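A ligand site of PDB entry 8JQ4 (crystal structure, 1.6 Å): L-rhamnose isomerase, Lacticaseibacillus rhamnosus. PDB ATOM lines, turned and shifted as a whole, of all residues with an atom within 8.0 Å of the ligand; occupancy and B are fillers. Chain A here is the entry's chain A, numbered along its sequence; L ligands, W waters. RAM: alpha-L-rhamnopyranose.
Water W4 bridges O4 of the ligand (2.6 Å) and OD2 of Asp 118 (3.0 Å). Water W1 bridges OD2 of Asp 122 (2.6 Å) and O3 of the ligand (2.7 Å). Water W3 bridges an oxygen (O1) of the ligand (2.7 Å) and the side-chain hydroxyl of Tyr 173 (2.8 Å). Water W2 bridges the side-chain carboxylate (OD2) of Asp 118 (2.5 Å) and an oxygen (O1) of the ligand (3.3 Å).
OD1 of Asp 118 is in hydrogen-bond range of OH of Tyr 173, 2.7 Å away. The backbone carbonyl oxygen (O) of Lys 177 sits at hydrogen-bond distance from the side-chain amino group (NZ) of Lys 125 (3.0 Å).
Residues that only touch the ligand: Asp 118 and Tyr 173. Within 4 Å of the ligand: Asp 118, Asp 122, Tyr 173 and Lys 177.
O4 of the ligand sits at hydrogen-bond distance from OD1 of Asp 122, 2.9 Å away. An oxygen (O5) of the ligand is in hydrogen-bond range of the side-chain amino group (NZ) of Lys 177, at 3.2 Å.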
ATOM      1  N   PRO A 114      -9.503 -14.180   5.719  1.00  0.00           N
ATOM      2  CA  PRO A 114      -9.579 -12.932   6.468  1.00  0.00           C
ATOM      3  C   PRO A 114     -10.966 -12.269   6.447  1.00  0.00           C
ATOM      4  O   PRO A 114     -11.400 -11.804   7.485  1.00  0.00           O
ATOM      5  CB  PRO A 114      -8.525 -12.058   5.779  1.00  0.00           C
ATOM      6  CG  PRO A 114      -7.501 -13.051   5.282  1.00  0.00           C
ATOM      7  CD  PRO A 114      -8.321 -14.243   4.841  1.00  0.00           C
ATOM      8  N   GLU A 115     -11.646 -12.265   5.294  1.00  0.00           N
ATOM      9  CA  GLU A 115     -12.927 -11.524   5.108  1.00  0.00           C
ATOM     10  C   GLU A 115     -14.039 -12.195   5.925  1.00  0.00           C
ATOM     11  O   GLU A 115     -15.098 -11.557   6.091  1.00  0.00           O
ATOM     12  CB  GLU A 115     -13.297 -11.409   3.629  1.00  0.00           C
ATOM     13  CG  GLU A 115     -13.545 -12.751   2.951  1.00  0.00           C
ATOM     14  CD  GLU A 115     -12.340 -13.307   2.209  1.00  0.00           C
ATOM     15  OE1 GLU A 115     -11.197 -12.994   2.606  1.00  0.00           O
ATOM     16  OE2 GLU A 115     -12.554 -14.079   1.255  1.00  0.00           O
ATOM     17  N   PHE A 117     -13.964 -12.325   8.865  1.00  0.00           N
ATOM     18  CA  PHE A 117     -13.903 -11.522  10.121  1.00  0.00           C
ATOM     19  C   PHE A 117     -14.278 -10.062   9.837  1.00  0.00           C
ATOM     20  O   PHE A 117     -14.185  -9.241  10.771  1.00  0.00           O
ATOM     21  CB  PHE A 117     -12.531 -11.695  10.790  1.00  0.00           C
ATOM     22  CG  PHE A 117     -12.330 -13.075  11.335  1.00  0.00           C
ATOM     23  CD1 PHE A 117     -12.764 -13.407  12.606  1.00  0.00           C
ATOM     24  CD2 PHE A 117     -11.841 -14.092  10.522  1.00  0.00           C
ATOM     25  CE1 PHE A 117     -12.642 -14.702  13.092  1.00  0.00           C
ATOM     26  CE2 PHE A 117     -11.734 -15.384  10.995  1.00  0.00           C
ATOM     27  CZ  PHE A 117     -12.124 -15.690  12.283  1.00  0.00           C
ATOM     28  N   ASP A 118     -14.792  -9.780   8.634  1.00  0.00           N
ATOM     29  CA  ASP A 118     -15.340  -8.456   8.239  1.00  0.00           C
ATOM     30  C   ASP A 118     -16.414  -8.025   9.246  1.00  0.00           C
ATOM     31  O   ASP A 118     -16.441  -6.829   9.608  1.00  0.00           O
ATOM     32  CB  ASP A 118     -15.921  -8.480   6.831  1.00  0.00           C
ATOM     33  CG  ASP A 118     -14.869  -8.480   5.748  1.00  0.00           C
ATOM     34  OD1 ASP A 118     -13.677  -8.345   6.109  1.00  0.00           O
ATOM     35  OD2 ASP A 118     -15.243  -8.592   4.557  1.00  0.00           O
ATOM     36  N   TYR A 119     -17.284  -8.948   9.672  1.00  0.00           N
ATOM     37  CA  TYR A 119     -18.379  -8.658  10.625  1.00  0.00           C
ATOM     38  C   TYR A 119     -17.776  -7.983  11.866  1.00  0.00           C
ATOM     39  O   TYR A 119     -18.327  -6.960  12.323  1.00  0.00           O
ATOM     40  CB  TYR A 119     -19.155  -9.922  11.004  1.00  0.00           C
ATOM     41  CG  TYR A 119     -20.225  -9.689  12.038  1.00  0.00           C
ATOM     42  CD1 TYR A 119     -21.536  -9.419  11.658  1.00  0.00           C
ATOM     43  CD2 TYR A 119     -19.930  -9.665  13.389  1.00  0.00           C
ATOM     44  CE1 TYR A 119     -22.519  -9.182  12.595  1.00  0.00           C
ATOM     45  CE2 TYR A 119     -20.906  -9.419  14.335  1.00  0.00           C
ATOM     46  CZ  TYR A 119     -22.211  -9.178  13.942  1.00  0.00           C
ATOM     47  OH  TYR A 119     -23.172  -8.919  14.874  1.00  0.00           O
ATOM     48  N   TRP A 120     -16.678  -8.534  12.377  1.00  0.00           N
ATOM     49  CA  TRP A 120     -16.051  -8.112  13.655  1.00  0.00           C
ATOM     50  C   TRP A 120     -15.235  -6.823  13.466  1.00  0.00           C
ATOM     51  O   TRP A 120     -15.213  -5.995  14.376  1.00  0.00           O
ATOM     52  CB  TRP A 120     -15.223  -9.241  14.266  1.00  0.00           C
ATOM     53  CG  TRP A 120     -16.084 -10.342  14.824  1.00  0.00           C
ATOM     54  CD1 TRP A 120     -16.155 -11.622  14.387  1.00  0.00           C
ATOM     55  CD2 TRP A 120     -17.087 -10.199  15.838  1.00  0.00           C
ATOM     56  NE1 TRP A 120     -17.119 -12.306  15.079  1.00  0.00           N
ATOM     57  CE2 TRP A 120     -17.706 -11.465  15.979  1.00  0.00           C
ATOM     58  CE3 TRP A 120     -17.526  -9.141  16.635  1.00  0.00           C
ATOM     59  CZ2 TRP A 120     -18.723 -11.693  16.910  1.00  0.00           C
ATOM     60  CZ3 TRP A 120     -18.522  -9.378  17.556  1.00  0.00           C
ATOM     61  CH2 TRP A 120     -19.121 -10.630  17.676  1.00  0.00           C
ATOM     62  N   ILE A 121     -14.623  -6.648  12.294  1.00  0.00           N
ATOM     63  CA  ILE A 121     -13.915  -5.368  11.950  1.00  0.00           C
ATOM     64  C   ILE A 121     -14.951  -4.248  11.924  1.00  0.00           C
ATOM     65  O   ILE A 121     -14.705  -3.193  12.555  1.00  0.00           O
ATOM     66  CB  ILE A 121     -13.164  -5.493  10.613  1.00  0.00           C
ATOM     67  CG1 ILE A 121     -11.977  -6.463  10.732  1.00  0.00           C
ATOM     68  CG2 ILE A 121     -12.732  -4.123  10.113  1.00  0.00           C
ATOM     69  CD1 ILE A 121     -11.388  -6.879   9.407  1.00  0.00           C
ATOM     70  N   ASP A 122     -16.072  -4.455  11.222  1.00  0.00           N
ATOM     71  CA  ASP A 122     -17.193  -3.493  11.135  1.00  0.00           C
ATOM     72  C   ASP A 122     -17.666  -3.169  12.552  1.00  0.00           C
ATOM     73  O   ASP A 122     -17.845  -1.970  12.872  1.00  0.00           O
ATOM     74  CB  ASP A 122     -18.345  -4.072  10.307  1.00  0.00           C
ATOM     75  CG  ASP A 122     -18.075  -4.140   8.811  1.00  0.00           C
ATOM     76  OD1 ASP A 122     -16.956  -3.786   8.388  1.00  0.00           O
ATOM     77  OD2 ASP A 122     -19.005  -4.541   8.077  1.00  0.00           O
ATOM     78  N   TRP A 123     -17.858  -4.193  13.393  1.00  0.00           N
ATOM     79  CA  TRP A 123     -18.372  -4.024  14.776  1.00  0.00           C
ATOM     80  C   TRP A 123     -17.371  -3.214  15.597  1.00  0.00           C
ATOM     81  O   TRP A 123     -17.803  -2.305  16.322  1.00  0.00           O
ATOM     82  CB  TRP A 123     -18.695  -5.366  15.434  1.00  0.00           C
ATOM     83  CG  TRP A 123     -19.179  -5.183  16.847  1.00  0.00           C
ATOM     84  CD1 TRP A 123     -20.430  -4.793  17.236  1.00  0.00           C
ATOM     85  CD2 TRP A 123     -18.391  -5.260  18.046  1.00  0.00           C
ATOM     86  NE1 TRP A 123     -20.485  -4.667  18.595  1.00  0.00           N
ATOM     87  CE2 TRP A 123     -19.252  -4.950  19.120  1.00  0.00           C
ATOM     88  CE3 TRP A 123     -17.060  -5.603  18.325  1.00  0.00           C
ATOM     89  CZ2 TRP A 123     -18.817  -4.956  20.444  1.00  0.00           C
ATOM     90  CZ3 TRP A 123     -16.640  -5.597  19.637  1.00  0.00           C
ATOM     91  CH2 TRP A 123     -17.502  -5.291  20.682  1.00  0.00           C
ATOM     92  N   LYS A 125     -15.075  -1.083  14.640  1.00  0.00           N
ATOM     93  CA  LYS A 125     -15.021   0.340  14.198  1.00  0.00           C
ATOM     94  C   LYS A 125     -16.202   1.109  14.776  1.00  0.00           C
ATOM     95  O   LYS A 125     -15.993   2.253  15.210  1.00  0.00           O
ATOM     96  CB  LYS A 125     -14.975   0.448  12.674  1.00  0.00           C
ATOM     97  CG  LYS A 125     -13.676  -0.043  12.055  1.00  0.00           C
ATOM     98  CD  LYS A 125     -13.436   0.461  10.661  1.00  0.00           C
ATOM     99  CE  LYS A 125     -11.991   0.275  10.236  1.00  0.00           C
ATOM    100  NZ  LYS A 125     -11.797   0.672   8.823  1.00  0.00           N
ATOM    101  N   TYR A 173      -4.706  -8.759   8.384  1.00  0.00           N
ATOM    102  CA  TYR A 173      -5.876  -8.142   7.695  1.00  0.00           C
ATOM    103  C   TYR A 173      -6.642  -7.260   8.684  1.00  0.00           C
ATOM    104  O   TYR A 173      -6.921  -6.091   8.362  1.00  0.00           O
ATOM    105  CB  TYR A 173      -6.752  -9.241   7.094  1.00  0.00           C
ATOM    106  CG  TYR A 173      -8.024  -8.789   6.437  1.00  0.00           C
ATOM    107  CD1 TYR A 173      -8.034  -8.294   5.140  1.00  0.00           C
ATOM    108  CD2 TYR A 173      -9.253  -8.935   7.077  1.00  0.00           C
ATOM    109  CE1 TYR A 173      -9.214  -7.913   4.515  1.00  0.00           C
ATOM    110  CE2 TYR A 173     -10.432  -8.566   6.464  1.00  0.00           C
ATOM    111  CZ  TYR A 173     -10.420  -8.053   5.176  1.00  0.00           C
ATOM    112  OH  TYR A 173     -11.585  -7.687   4.577  1.00  0.00           O
ATOM    113  N   ILE A 174      -7.002  -7.810   9.853  1.00  0.00           N
ATOM    114  CA  ILE A 174      -7.739  -7.052  10.903  1.00  0.00           C
ATOM    115  C   ILE A 174      -6.907  -5.821  11.293  1.00  0.00           C
ATOM    116  O   ILE A 174      -7.485  -4.723  11.355  1.00  0.00           O
ATOM    117  CB  ILE A 174      -8.062  -7.938  12.122  1.00  0.00           C
ATOM    118  CG1 ILE A 174      -9.032  -9.068  11.759  1.00  0.00           C
ATOM    119  CG2 ILE A 174      -8.565  -7.096  13.278  1.00  0.00           C
ATOM    120  CD1 ILE A 174      -9.257 -10.060  12.874  1.00  0.00           C
ATOM    121  N   LYS A 177      -6.922  -3.090   8.643  1.00  0.00           N
ATOM    122  CA  LYS A 177      -8.265  -2.453   8.535  1.00  0.00           C
ATOM    123  C   LYS A 177      -8.515  -1.528   9.743  1.00  0.00           C
ATOM    124  O   LYS A 177      -9.051  -0.431   9.529  1.00  0.00           O
ATOM    125  CB  LYS A 177      -9.346  -3.525   8.432  1.00  0.00           C
ATOM    126  CG  LYS A 177      -9.368  -4.287   7.110  1.00  0.00           C
ATOM    127  CD  LYS A 177      -9.715  -3.398   5.947  1.00  0.00           C
ATOM    128  CE  LYS A 177      -9.975  -4.158   4.665  1.00  0.00           C
ATOM    129  NZ  LYS A 177     -10.416  -3.250   3.583  1.00  0.00           N
ATOM    130  N   LEU A 178      -8.133  -1.969  10.952  1.00  0.00           N
ATOM    131  CA  LEU A 178      -8.441  -1.236  12.214  1.00  0.00           C
ATOM    132  C   LEU A 178      -7.401  -0.138  12.461  1.00  0.00           C
ATOM    133  O   LEU A 178      -7.756   0.850  13.132  1.00  0.00           O
ATOM    134  CB  LEU A 178      -8.458  -2.225  13.384  1.00  0.00           C
ATOM    135  CG  LEU A 178      -9.662  -3.169  13.435  1.00  0.00           C
ATOM    136  CD1 LEU A 178      -9.705  -3.893  14.771  1.00  0.00           C
ATOM    137  CD2 LEU A 178     -10.974  -2.426  13.194  1.00  0.00           C
HETATM  138  C1  RAM L   1     -13.912  -4.057   2.731  1.00  0.00           C
HETATM  139  C2  RAM L   1     -15.235  -3.292   2.811  1.00  0.00           C
HETATM  140  C3  RAM L   1     -16.226  -4.057   3.669  1.00  0.00           C
HETATM  141  C4  RAM L   1     -15.626  -4.332   5.035  1.00  0.00           C
HETATM  142  C5  RAM L   1     -14.284  -5.046   4.898  1.00  0.00           C
HETATM  143  C6  RAM L   1     -13.605  -5.230   6.255  1.00  0.00           C
HETATM  144  O1  RAM L   1     -14.131  -5.295   2.042  1.00  0.00           O
HETATM  145  O2  RAM L   1     -15.007  -1.992   3.382  1.00  0.00           O
HETATM  146  O3  RAM L   1     -17.439  -3.309   3.820  1.00  0.00           O
HETATM  147  O4  RAM L   1     -16.558  -5.096   5.825  1.00  0.00           O
HETATM  148  O5  RAM L   1     -13.399  -4.309   4.048  1.00  0.00           O
HETATM  149  O   HOH W   1     -19.217  -3.188   5.813  1.00  0.00           O
HETATM  150  O   HOH W   2     -14.720  -8.583   2.105  1.00  0.00           O
HETATM  151  O   HOH W   3     -11.901  -6.885   1.955  1.00  0.00           O
HETATM  152  O   HOH W   4     -17.822  -7.083   4.762  1.00  0.00           O
